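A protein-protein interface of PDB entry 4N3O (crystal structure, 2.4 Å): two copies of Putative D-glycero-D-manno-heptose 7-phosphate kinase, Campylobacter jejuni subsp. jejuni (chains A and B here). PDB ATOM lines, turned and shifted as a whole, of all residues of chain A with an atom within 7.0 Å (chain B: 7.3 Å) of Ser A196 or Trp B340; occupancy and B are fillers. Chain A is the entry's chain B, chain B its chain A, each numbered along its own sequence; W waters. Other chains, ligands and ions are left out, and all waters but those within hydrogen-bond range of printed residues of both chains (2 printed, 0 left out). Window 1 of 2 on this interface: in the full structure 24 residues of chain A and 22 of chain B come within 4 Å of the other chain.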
ATOM      1  N   ILE A 190     -11.587   1.717 -16.163  1.00  0.00           N
ATOM      2  CA  ILE A 190     -12.662   1.184 -16.957  1.00  0.00           C
ATOM      3  C   ILE A 190     -12.804   2.070 -18.181  1.00  0.00           C
ATOM      4  O   ILE A 190     -12.883   3.299 -18.044  1.00  0.00           O
ATOM      5  CB  ILE A 190     -13.967   1.255 -16.138  1.00  0.00           C
ATOM      6  CG1 ILE A 190     -13.906   0.285 -14.960  1.00  0.00           C
ATOM      7  CG2 ILE A 190     -15.174   0.931 -16.991  1.00  0.00           C
ATOM      8  CD1 ILE A 190     -13.827  -1.170 -15.370  1.00  0.00           C
ATOM      9  N   LYS A 191     -12.840   1.467 -19.368  1.00  0.00           N
ATOM     10  CA  LYS A 191     -13.029   2.248 -20.597  1.00  0.00           C
ATOM     11  C   LYS A 191     -14.337   3.012 -20.463  1.00  0.00           C
ATOM     12  O   LYS A 191     -15.340   2.452 -20.002  1.00  0.00           O
ATOM     13  CB  LYS A 191     -13.140   1.362 -21.840  1.00  0.00           C
ATOM     14  CG  LYS A 191     -11.978   0.430 -22.131  1.00  0.00           C
ATOM     15  CD  LYS A 191     -12.310  -0.367 -23.384  1.00  0.00           C
ATOM     16  CE  LYS A 191     -11.392  -1.560 -23.606  1.00  0.00           C
ATOM     17  NZ  LYS A 191     -11.889  -2.381 -24.754  1.00  0.00           N
ATOM     18  N   ASN A 192     -14.326   4.274 -20.879  1.00  0.00           N
ATOM     19  CA  ASN A 192     -15.499   5.132 -20.802  1.00  0.00           C
ATOM     20  C   ASN A 192     -16.793   4.534 -21.345  1.00  0.00           C
ATOM     21  O   ASN A 192     -17.846   4.598 -20.688  1.00  0.00           O
ATOM     22  CB  ASN A 192     -15.211   6.483 -21.464  1.00  0.00           C
ATOM     23  CG  ASN A 192     -14.292   7.362 -20.615  1.00  0.00           C
ATOM     24  OD1 ASN A 192     -13.761   6.933 -19.575  1.00  0.00           O
ATOM     25  ND2 ASN A 192     -14.109   8.593 -21.042  1.00  0.00           N
ATOM     26  N   TRP A 193     -16.722   3.903 -22.504  1.00  0.00           N
ATOM     27  CA  TRP A 193     -17.928   3.340 -23.076  1.00  0.00           C
ATOM     28  C   TRP A 193     -18.550   2.239 -22.224  1.00  0.00           C
ATOM     29  O   TRP A 193     -19.751   1.984 -22.330  1.00  0.00           O
ATOM     30  CB  TRP A 193     -17.698   2.879 -24.511  1.00  0.00           C
ATOM     31  CG  TRP A 193     -16.915   1.653 -24.663  1.00  0.00           C
ATOM     32  CD1 TRP A 193     -15.563   1.559 -24.867  1.00  0.00           C
ATOM     33  CD2 TRP A 193     -17.420   0.318 -24.644  1.00  0.00           C
ATOM     34  NE1 TRP A 193     -15.196   0.231 -24.973  1.00  0.00           N
ATOM     35  CE2 TRP A 193     -16.315  -0.550 -24.845  1.00  0.00           C
ATOM     36  CE3 TRP A 193     -18.692  -0.238 -24.446  1.00  0.00           C
ATOM     37  CZ2 TRP A 193     -16.450  -1.937 -24.872  1.00  0.00           C
ATOM     38  CZ3 TRP A 193     -18.833  -1.624 -24.476  1.00  0.00           C
ATOM     39  CH2 TRP A 193     -17.719  -2.458 -24.694  1.00  0.00           C
ATOM     40  N   ILE A 194     -17.760   1.574 -21.381  1.00  0.00           N
ATOM     41  CA  ILE A 194     -18.335   0.535 -20.502  1.00  0.00           C
ATOM     42  C   ILE A 194     -19.287   1.191 -19.510  1.00  0.00           C
ATOM     43  O   ILE A 194     -20.392   0.730 -19.313  1.00  0.00           O
ATOM     44  CB  ILE A 194     -17.262  -0.268 -19.754  1.00  0.00           C
ATOM     45  CG1 ILE A 194     -16.412  -1.043 -20.771  1.00  0.00           C
ATOM     46  CG2 ILE A 194     -17.918  -1.224 -18.768  1.00  0.00           C
ATOM     47  CD1 ILE A 194     -15.295  -1.879 -20.165  1.00  0.00           C
ATOM     48  N   ALA A 195     -18.826   2.262 -18.884  1.00  0.00           N
ATOM     49  CA  ALA A 195     -19.649   3.036 -17.961  1.00  0.00           C
ATOM     50  C   ALA A 195     -20.877   3.572 -18.706  1.00  0.00           C
ATOM     51  O   ALA A 195     -21.988   3.557 -18.181  1.00  0.00           O
ATOM     52  CB  ALA A 195     -18.848   4.202 -17.395  1.00  0.00           C
ATOM     53  N   SER A 196     -20.662   4.039 -19.934  1.00  0.00           N
ATOM     54  CA  SER A 196     -21.735   4.596 -20.724  1.00  0.00           C
ATOM     55  C   SER A 196     -22.796   3.569 -21.037  1.00  0.00           C
ATOM     56  O   SER A 196     -23.988   3.887 -20.987  1.00  0.00           O
ATOM     57  CB  SER A 196     -21.200   5.195 -22.020  1.00  0.00           C
ATOM     58  OG  SER A 196     -20.357   6.285 -21.739  1.00  0.00           O
ATOM     59  N   GLU A 197     -22.367   2.345 -21.368  1.00  0.00           N
ATOM     60  CA  GLU A 197     -23.293   1.262 -21.664  1.00  0.00           C
ATOM     61  C   GLU A 197     -24.030   0.855 -20.392  1.00  0.00           C
ATOM     62  O   GLU A 197     -25.224   0.597 -20.416  1.00  0.00           O
ATOM     63  CB  GLU A 197     -22.540   0.075 -22.251  1.00  0.00           C
ATOM     64  CG  GLU A 197     -23.398  -1.148 -22.595  1.00  0.00           C
ATOM     65  CD  GLU A 197     -24.437  -0.876 -23.667  1.00  0.00           C
ATOM     66  OE1 GLU A 197     -24.229   0.041 -24.479  1.00  0.00           O
ATOM     67  OE2 GLU A 197     -25.465  -1.602 -23.713  1.00  0.00           O
ATOM     68  N   LEU A 198     -23.316   0.786 -19.275  1.00  0.00           N
ATOM     69  CA  LEU A 198     -23.960   0.457 -18.021  1.00  0.00           C
ATOM     70  C   LEU A 198     -25.020   1.491 -17.695  1.00  0.00           C
ATOM     71  O   LEU A 198     -26.125   1.120 -17.333  1.00  0.00           O
ATOM     72  CB  LEU A 198     -22.958   0.349 -16.890  1.00  0.00           C
ATOM     73  CG  LEU A 198     -22.353  -1.031 -16.677  1.00  0.00           C
ATOM     74  CD1 LEU A 198     -21.190  -0.959 -15.703  1.00  0.00           C
ATOM     75  CD2 LEU A 198     -23.422  -1.991 -16.146  1.00  0.00           C
ATOM     76  N   GLU A 199     -24.689   2.781 -17.837  1.00  0.00           N
ATOM     77  CA  GLU A 199     -25.659   3.874 -17.585  1.00  0.00           C
ATOM     78  C   GLU A 199     -26.862   3.778 -18.513  1.00  0.00           C
ATOM     79  O   GLU A 199     -27.973   4.047 -18.096  1.00  0.00           O
ATOM     80  CB  GLU A 199     -25.024   5.236 -17.803  1.00  0.00           C
ATOM     81  CG  GLU A 199     -23.911   5.548 -16.831  1.00  0.00           C
ATOM     82  CD  GLU A 199     -22.960   6.623 -17.336  1.00  0.00           C
ATOM     83  OE1 GLU A 199     -23.211   7.204 -18.403  1.00  0.00           O
ATOM     84  OE2 GLU A 199     -21.951   6.879 -16.663  1.00  0.00           O
ATOM     85  N   ALA A 200     -26.626   3.441 -19.783  1.00  0.00           N
ATOM     86  CA  ALA A 200     -27.710   3.307 -20.748  1.00  0.00           C
ATOM     87  C   ALA A 200     -28.673   2.180 -20.374  1.00  0.00           C
ATOM     88  O   ALA A 200     -29.834   2.240 -20.759  1.00  0.00           O
ATOM     89  CB  ALA A 200     -27.166   3.048 -22.129  1.00  0.00           C
ATOM     90  N   ARG A 201     -28.196   1.174 -19.628  1.00  0.00           N
ATOM     91  CA  ARG A 201     -29.040   0.043 -19.222  1.00  0.00           C
ATOM     92  C   ARG A 201     -29.545   0.141 -17.807  1.00  0.00           C
ATOM     93  O   ARG A 201     -30.089  -0.813 -17.289  1.00  0.00           O
ATOM     94  CB  ARG A 201     -28.248  -1.253 -19.245  1.00  0.00           C
ATOM     95  CG  ARG A 201     -27.511  -1.535 -20.503  1.00  0.00           C
ATOM     96  CD  ARG A 201     -27.026  -2.948 -20.474  1.00  0.00           C
ATOM     97  NE  ARG A 201     -26.274  -3.252 -21.679  1.00  0.00           N
ATOM     98  CZ  ARG A 201     -26.018  -4.480 -22.103  1.00  0.00           C
ATOM     99  NH1 ARG A 201     -26.494  -5.523 -21.437  1.00  0.00           N
ATOM    100  NH2 ARG A 201     -25.319  -4.660 -23.218  1.00  0.00           N
ATOM    101  N   PHE A 252     -19.809  -7.476 -22.097  1.00  0.00           N
ATOM    102  CA  PHE A 252     -21.101  -7.195 -21.502  1.00  0.00           C
ATOM    103  C   PHE A 252     -21.986  -8.377 -21.337  1.00  0.00           C
ATOM    104  O   PHE A 252     -22.743  -8.432 -20.353  1.00  0.00           O
ATOM    105  CB  PHE A 252     -21.827  -6.062 -22.213  1.00  0.00           C
ATOM    106  CG  PHE A 252     -21.621  -4.770 -21.549  1.00  0.00           C
ATOM    107  CD1 PHE A 252     -22.433  -4.411 -20.499  1.00  0.00           C
ATOM    108  CD2 PHE A 252     -20.571  -3.950 -21.902  1.00  0.00           C
ATOM    109  CE1 PHE A 252     -22.233  -3.233 -19.826  1.00  0.00           C
ATOM    110  CE2 PHE A 252     -20.360  -2.759 -21.231  1.00  0.00           C
ATOM    111  CZ  PHE A 252     -21.196  -2.401 -20.197  1.00  0.00           C
ATOM    112  N   PHE A 332     -21.827   7.483 -13.910  1.00  0.00           N
ATOM    113  CA  PHE A 332     -20.716   7.046 -13.110  1.00  0.00           C
ATOM    114  C   PHE A 332     -19.636   8.126 -13.246  1.00  0.00           C
ATOM    115  O   PHE A 332     -19.388   8.624 -14.350  1.00  0.00           O
ATOM    116  CB  PHE A 332     -20.212   5.676 -13.583  1.00  0.00           C
ATOM    117  CG  PHE A 332     -21.201   4.567 -13.356  1.00  0.00           C
ATOM    118  CD1 PHE A 332     -21.458   4.098 -12.061  1.00  0.00           C
ATOM    119  CD2 PHE A 332     -21.884   3.994 -14.410  1.00  0.00           C
ATOM    120  CE1 PHE A 332     -22.376   3.076 -11.838  1.00  0.00           C
ATOM    121  CE2 PHE A 332     -22.799   2.970 -14.197  1.00  0.00           C
ATOM    122  CZ  PHE A 332     -23.053   2.519 -12.908  1.00  0.00           C
ATOM    123  N   LYS A 334     -15.646   9.601 -12.622  1.00  0.00           N
ATOM    124  CA  LYS A 334     -14.293   9.059 -12.714  1.00  0.00           C
ATOM    125  C   LYS A 334     -13.476   9.328 -11.477  1.00  0.00           C
ATOM    126  O   LYS A 334     -12.533   8.609 -11.215  1.00  0.00           O
ATOM    127  CB  LYS A 334     -13.548   9.632 -13.927  1.00  0.00           C
ATOM    128  CG  LYS A 334     -14.084   9.194 -15.283  1.00  0.00           C
ATOM    129  CD  LYS A 334     -15.465   9.761 -15.582  1.00  0.00           C
ATOM    130  CE  LYS A 334     -15.951   9.398 -16.985  1.00  0.00           C
ATOM    131  NZ  LYS A 334     -16.226   7.942 -17.154  1.00  0.00           N
ATOM    132  N   THR B   6     -24.769  -3.216 -32.924  1.00  0.00           N
ATOM    133  CA  THR B   6     -25.550  -2.153 -32.304  1.00  0.00           C
ATOM    134  C   THR B   6     -24.666  -0.945 -32.062  1.00  0.00           C
ATOM    135  O   THR B   6     -23.546  -1.079 -31.567  1.00  0.00           O
ATOM    136  CB  THR B   6     -26.105  -2.597 -30.941  1.00  0.00           C
ATOM    137  OG1 THR B   6     -26.856  -3.795 -31.108  1.00  0.00           O
ATOM    138  CG2 THR B   6     -26.995  -1.538 -30.351  1.00  0.00           C
ATOM    139  N   ILE B   7     -25.165   0.230 -32.408  1.00  0.00           N
ATOM    140  CA  ILE B   7     -24.412   1.463 -32.209  1.00  0.00           C
ATOM    141  C   ILE B   7     -25.247   2.316 -31.290  1.00  0.00           C
ATOM    142  O   ILE B   7     -26.464   2.349 -31.425  1.00  0.00           O
ATOM    143  CB  ILE B   7     -24.238   2.241 -33.531  1.00  0.00           C
ATOM    144  CG1 ILE B   7     -23.374   1.452 -34.527  1.00  0.00           C
ATOM    145  CG2 ILE B   7     -23.651   3.636 -33.290  1.00  0.00           C
ATOM    146  CD1 ILE B   7     -21.897   1.412 -34.205  1.00  0.00           C
ATOM    147  N   ARG B   8     -24.601   2.987 -30.342  1.00  0.00           N
ATOM    148  CA  ARG B   8     -25.320   3.881 -29.483  1.00  0.00           C
ATOM    149  C   ARG B   8     -24.589   5.190 -29.505  1.00  0.00           C
ATOM    150  O   ARG B   8     -23.368   5.211 -29.683  1.00  0.00           O
ATOM    151  CB  ARG B   8     -25.379   3.385 -28.030  1.00  0.00           C
ATOM    152  CG  ARG B   8     -25.980   1.991 -27.816  1.00  0.00           C
ATOM    153  CD  ARG B   8     -26.504   1.844 -26.394  1.00  0.00           C
ATOM    154  NE  ARG B   8     -26.530   0.455 -25.973  1.00  0.00           N
ATOM    155  CZ  ARG B   8     -27.475  -0.422 -26.307  1.00  0.00           C
ATOM    156  NH1 ARG B   8     -27.365  -1.661 -25.883  1.00  0.00           N
ATOM    157  NH2 ARG B   8     -28.508  -0.078 -27.084  1.00  0.00           N
ATOM    158  N   THR B   9     -25.333   6.280 -29.350  1.00  0.00           N
ATOM    159  CA  THR B   9     -24.720   7.593 -29.221  1.00  0.00           C
ATOM    160  C   THR B   9     -25.440   8.351 -28.097  1.00  0.00           C
ATOM    161  O   THR B   9     -26.636   8.118 -27.800  1.00  0.00           O
ATOM    162  CB  THR B   9     -24.723   8.440 -30.524  1.00  0.00           C
ATOM    163  OG1 THR B   9     -26.037   8.896 -30.822  1.00  0.00           O
ATOM    164  CG2 THR B   9     -24.192   7.652 -31.688  1.00  0.00           C
ATOM    165  N   GLN B  10     -24.698   9.263 -27.494  1.00  0.00           N
ATOM    166  CA  GLN B  10     -25.187  10.089 -26.398  1.00  0.00           C
ATOM    167  C   GLN B  10     -24.671  11.500 -26.699  1.00  0.00           C
ATOM    168  O   GLN B  10     -23.469  11.706 -26.901  1.00  0.00           O
ATOM    169  CB  GLN B  10     -24.655   9.529 -25.089  1.00  0.00           C
ATOM    170  CG  GLN B  10     -25.094  10.293 -23.871  1.00  0.00           C
ATOM    171  CD  GLN B  10     -24.645   9.646 -22.562  1.00  0.00           C
ATOM    172  OE1 GLN B  10     -24.051   8.554 -22.536  1.00  0.00           O
ATOM    173  NE2 GLN B  10     -24.941  10.318 -21.469  1.00  0.00           N
ATOM    174  N   THR B  11     -25.584  12.457 -26.742  1.00  0.00           N
ATOM    175  CA  THR B  11     -25.279  13.810 -27.148  1.00  0.00           C
ATOM    176  C   THR B  11     -25.847  14.766 -26.126  1.00  0.00           C
ATOM    177  O   THR B  11     -27.018  14.706 -25.805  1.00  0.00           O
ATOM    178  CB  THR B  11     -25.950  14.080 -28.515  1.00  0.00           C
ATOM    179  OG1 THR B  11     -25.650  13.002 -29.430  1.00  0.00           O
ATOM    180  CG2 THR B  11     -25.504  15.424 -29.101  1.00  0.00           C
ATOM    181  N   HIS B  45     -30.423  10.318 -26.336  1.00  0.00           N
ATOM    182  CA  HIS B  45     -29.864   8.992 -26.456  1.00  0.00           C
ATOM    183  C   HIS B  45     -30.353   8.385 -27.747  1.00  0.00           C
ATOM    184  O   HIS B  45     -31.519   8.488 -28.068  1.00  0.00           O
ATOM    185  CB  HIS B  45     -30.329   8.115 -25.279  1.00  0.00           C
ATOM    186  CG  HIS B  45     -30.178   8.770 -23.946  1.00  0.00           C
ATOM    187  ND1 HIS B  45     -29.069   8.589 -23.152  1.00  0.00           N
ATOM    188  CD2 HIS B  45     -30.985   9.633 -23.275  1.00  0.00           C
ATOM    189  CE1 HIS B  45     -29.198   9.309 -22.049  1.00  0.00           C
ATOM    190  NE2 HIS B  45     -30.354   9.946 -22.096  1.00  0.00           N
ATOM    191  N   CYS B  46     -29.449   7.755 -28.485  1.00  0.00           N
ATOM    192  CA  CYS B  46     -29.791   7.098 -29.741  1.00  0.00           C
ATOM    193  C   CYS B  46     -29.193   5.709 -29.807  1.00  0.00           C
ATOM    194  O   CYS B  46     -28.034   5.512 -29.450  1.00  0.00           O
ATOM    195  CB  CYS B  46     -29.263   7.884 -30.949  1.00  0.00           C
ATOM    196  SG  CYS B  46     -29.979   9.528 -31.146  1.00  0.00           S
ATOM    197  N   THR B  47     -29.997   4.755 -30.257  1.00  0.00           N
ATOM    198  CA  THR B  47     -29.543   3.393 -30.480  1.00  0.00           C
ATOM    199  C   THR B  47     -29.888   3.039 -31.939  1.00  0.00           C
ATOM    200  O   THR B  47     -31.035   3.215 -32.381  1.00  0.00           O
ATOM    201  CB  THR B  47     -30.201   2.389 -29.536  1.00  0.00           C
ATOM    202  OG1 THR B  47     -29.639   2.534 -28.237  1.00  0.00           O
ATOM    203  CG2 THR B  47     -29.932   0.999 -29.986  1.00  0.00           C
ATOM    204  N   LYS B 128     -24.313  10.958 -36.106  1.00  0.00           N
ATOM    205  CA  LYS B 128     -23.149  10.280 -35.501  1.00  0.00           C
ATOM    206  C   LYS B 128     -23.341   8.780 -35.427  1.00  0.00           C
ATOM    207  O   LYS B 128     -22.395   8.022 -35.554  1.00  0.00           O
ATOM    208  CB  LYS B 128     -22.896  10.838 -34.104  1.00  0.00           C
ATOM    209  CG  LYS B 128     -21.693  10.259 -33.398  1.00  0.00           C
ATOM    210  CD  LYS B 128     -20.368  10.588 -34.068  1.00  0.00           C
ATOM    211  CE  LYS B 128     -19.251   9.936 -33.290  1.00  0.00           C
ATOM    212  NZ  LYS B 128     -17.937  10.192 -33.907  1.00  0.00           N
ATOM    213  N   GLU B 132     -20.683   6.261 -37.386  1.00  0.00           N
ATOM    214  CA  GLU B 132     -19.997   5.221 -36.622  1.00  0.00           C
ATOM    215  C   GLU B 132     -20.288   3.835 -37.189  1.00  0.00           C
ATOM    216  O   GLU B 132     -19.401   2.987 -37.309  1.00  0.00           O
ATOM    217  CB  GLU B 132     -20.508   5.259 -35.182  1.00  0.00           C
ATOM    218  CG  GLU B 132     -19.890   4.248 -34.232  1.00  0.00           C
ATOM    219  CD  GLU B 132     -18.497   4.634 -33.786  1.00  0.00           C
ATOM    220  OE1 GLU B 132     -17.762   5.244 -34.590  1.00  0.00           O
ATOM    221  OE2 GLU B 132     -18.144   4.321 -32.634  1.00  0.00           O
ATOM    222  N   GLU B 335     -17.192  16.667 -22.827  1.00  0.00           N
ATOM    223  CA  GLU B 335     -17.351  16.103 -24.152  1.00  0.00           C
ATOM    224  C   GLU B 335     -18.614  16.507 -24.871  1.00  0.00           C
ATOM    225  O   GLU B 335     -19.616  16.877 -24.267  1.00  0.00           O
ATOM    226  CB  GLU B 335     -17.371  14.557 -24.080  1.00  0.00           C
ATOM    227  CG  GLU B 335     -16.027  13.856 -24.211  1.00  0.00           C
ATOM    228  CD  GLU B 335     -16.178  12.339 -24.387  1.00  0.00           C
ATOM    229  OE1 GLU B 335     -16.730  11.673 -23.480  1.00  0.00           O
ATOM    230  OE2 GLU B 335     -15.723  11.806 -25.428  1.00  0.00           O
ATOM    231  N   LYS B 338     -20.772  11.391 -28.039  1.00  0.00           N
ATOM    232  CA  LYS B 338     -19.912  10.211 -27.947  1.00  0.00           C
ATOM    233  C   LYS B 338     -20.682   9.015 -28.522  1.00  0.00           C
ATOM    234  O   LYS B 338     -21.899   9.014 -28.545  1.00  0.00           O
ATOM    235  CB  LYS B 338     -19.422   9.908 -26.518  1.00  0.00           C
ATOM    236  CG  LYS B 338     -20.440   9.307 -25.562  1.00  0.00           C
ATOM    237  CD  LYS B 338     -20.953  10.278 -24.516  1.00  0.00           C
ATOM    238  CE  LYS B 338     -19.892  10.499 -23.454  1.00  0.00           C
ATOM    239  NZ  LYS B 338     -20.401  11.371 -22.372  1.00  0.00           N
ATOM    240  N   SER B 339     -19.966   8.018 -29.010  1.00  0.00           N
ATOM    241  CA  SER B 339     -20.604   6.833 -29.556  1.00  0.00           C
ATOM    242  C   SER B 339     -19.790   5.618 -29.258  1.00  0.00           C
ATOM    243  O   SER B 339     -18.595   5.713 -29.051  1.00  0.00           O
ATOM    244  CB  SER B 339     -20.703   6.932 -31.065  1.00  0.00           C
ATOM    245  OG  SER B 339     -19.404   6.983 -31.569  1.00  0.00           O
ATOM    246  N   TRP B 340     -20.447   4.469 -29.274  1.00  0.00           N
ATOM    247  CA  TRP B 340     -19.786   3.201 -29.049  1.00  0.00           C
ATOM    248  C   TRP B 340     -20.587   2.103 -29.705  1.00  0.00           C
ATOM    249  O   TRP B 340     -21.760   2.274 -30.006  1.00  0.00           O
ATOM    250  CB  TRP B 340     -19.588   2.931 -27.546  1.00  0.00           C
ATOM    251  CG  TRP B 340     -20.860   2.825 -26.695  1.00  0.00           C
ATOM    252  CD1 TRP B 340     -21.463   1.675 -26.274  1.00  0.00           C
ATOM    253  CD2 TRP B 340     -21.623   3.901 -26.132  1.00  0.00           C
ATOM    254  NE1 TRP B 340     -22.547   1.963 -25.485  1.00  0.00           N
ATOM    255  CE2 TRP B 340     -22.666   3.325 -25.376  1.00  0.00           C
ATOM    256  CE3 TRP B 340     -21.526   5.293 -26.189  1.00  0.00           C
ATOM    257  CZ2 TRP B 340     -23.624   4.094 -24.711  1.00  0.00           C
ATOM    258  CZ3 TRP B 340     -22.476   6.061 -25.511  1.00  0.00           C
ATOM    259  CH2 TRP B 340     -23.505   5.460 -24.785  1.00  0.00           C
ATOM    260  N   ARG B 341     -19.918   0.983 -29.934  1.00  0.00           N
ATOM    261  CA  ARG B 341     -20.475  -0.174 -30.601  1.00  0.00           C
ATOM    262  C   ARG B 341     -20.536  -1.277 -29.556  1.00  0.00           C
ATOM    263  O   ARG B 341     -19.641  -1.391 -28.733  1.00  0.00           O
ATOM    264  CB  ARG B 341     -19.529  -0.553 -31.736  1.00  0.00           C
ATOM    265  CG  ARG B 341     -20.141  -1.309 -32.895  1.00  0.00           C
ATOM    266  CD  ARG B 341     -19.082  -1.627 -33.950  1.00  0.00           C
ATOM    267  NE  ARG B 341     -19.661  -1.728 -35.295  1.00  0.00           N
ATOM    268  CZ  ARG B 341     -19.585  -0.780 -36.244  1.00  0.00           C
ATOM    269  NH1 ARG B 341     -20.167  -0.991 -37.423  1.00  0.00           N
ATOM    270  NH2 ARG B 341     -18.927   0.372 -36.042  1.00  0.00           N
ATOM    271  N   ILE B 342     -21.593  -2.071 -29.568  1.00  0.00           N
ATOM    272  CA  ILE B 342     -21.741  -3.138 -28.592  1.00  0.00           C
ATOM    273  C   ILE B 342     -22.371  -4.344 -29.294  1.00  0.00           C
ATOM    274  O   ILE B 342     -22.170  -5.494 -28.914  1.00  0.00           O
ATOM    275  CB  ILE B 342     -22.581  -2.640 -27.381  1.00  0.00           C
ATOM    276  CG1 ILE B 342     -22.307  -3.456 -26.099  1.00  0.00           C
ATOM    277  CG2 ILE B 342     -24.065  -2.532 -27.746  1.00  0.00           C
ATOM    278  CD1 ILE B 342     -22.754  -4.901 -26.125  1.00  0.00           C
ATOM    279  OXT ILE B 342     -23.075  -4.219 -30.298  1.00  0.00           O
HETATM  280  O   HOH W   1     -25.144   6.356 -21.706  1.00  0.00           O
HETATM  281  O   HOH W   2     -21.812   8.137 -20.701  1.00  0.00           O
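The indole nitrogen (NE1) of Trp B340 is in hydrogen-bond range of the side-chain carboxylate (OE1) of Glu A197 (2.7 Å).
The guanidinium group of Arg B8 lies within salt-bridge range of the side-chain carboxylate of Glu A197 (2.8 Å).
The backbone carbonyl oxygen (O) of Asn A192 sits at hydrogen-bond distance from the side-chain hydroxyl (OG) of Ser A196, at 3.2 Å.
NE of Arg A201 is in salt-bridge range of OE2 of Glu A197 (2.7 Å).
The backbone NH (N) of Arg B8 lies within hydrogen-bond range of the backbone carbonyl oxygen (O) of Trp B340.
The backbone NH (N) of Ile B342 lies within hydrogen-bond range of the backbone carbonyl oxygen (O) of Thr B6 (3.0 Å).
OG1 of Thr B47 lies within hydrogen-bond range of NH2 of Arg B8, 3.1 Å away.
Among the printed residues, pairs that only touch across the chains: Trp A193 with Trp B340 (3.6 Å), Ser A196 with Trp B340 (3.6 Å) and Arg A201 with Ile B342 (3.9 Å).
Ile A194 touches none of the printed residues of chain B.
No residue of chain B comes within 4 Å of Ala A195.
Ser A196 touches just one residue of chain B: Trp B340 (3.6 Å).
Printed residues of chain B within 4 Å of Glu A197: Arg B8 (2.8 Å) and Trp B340 (2.7 Å).
Of the printed residues of chain B, Arg A201 touches Ile B342 (3.9 Å).
Ile B7 touches none of the printed residues of chain A.
Of the printed residues of chain A, Arg B8 touches Glu A197.
Trp B340 touches just these residues of chain A: Trp A193 (3.6 Å), Ser A196 (3.6 Å) and Glu A197 (2.7 Å).
Printed residues of chain A within 4 Å of Ile B342: Arg A201.
Of the 15 printed residues of chain A, 4 touch a printed residue of chain B.
Printed residues of chain A that touch a printed residue of chain B: Trp A193, Ser A196, Glu A197 and Arg A201.
No position is printed for both chains.
Of the 5 pairs that touch across the chains among the printed residues, none has its exchanged pair printed and touching as well.
Water W2 lies within hydrogen-bond range of the side-chain hydroxyl of Ser A196 (2.6 Å), the side-chain carboxylate of Glu A199 (2.8 Å) and the side-chain amide oxygen of Gln B10 (2.9 Å).
Water W1 lies within hydrogen-bond range of the side-chain amide oxygen of Gln B10 and the backbone carbonyl oxygen of Ser A196.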
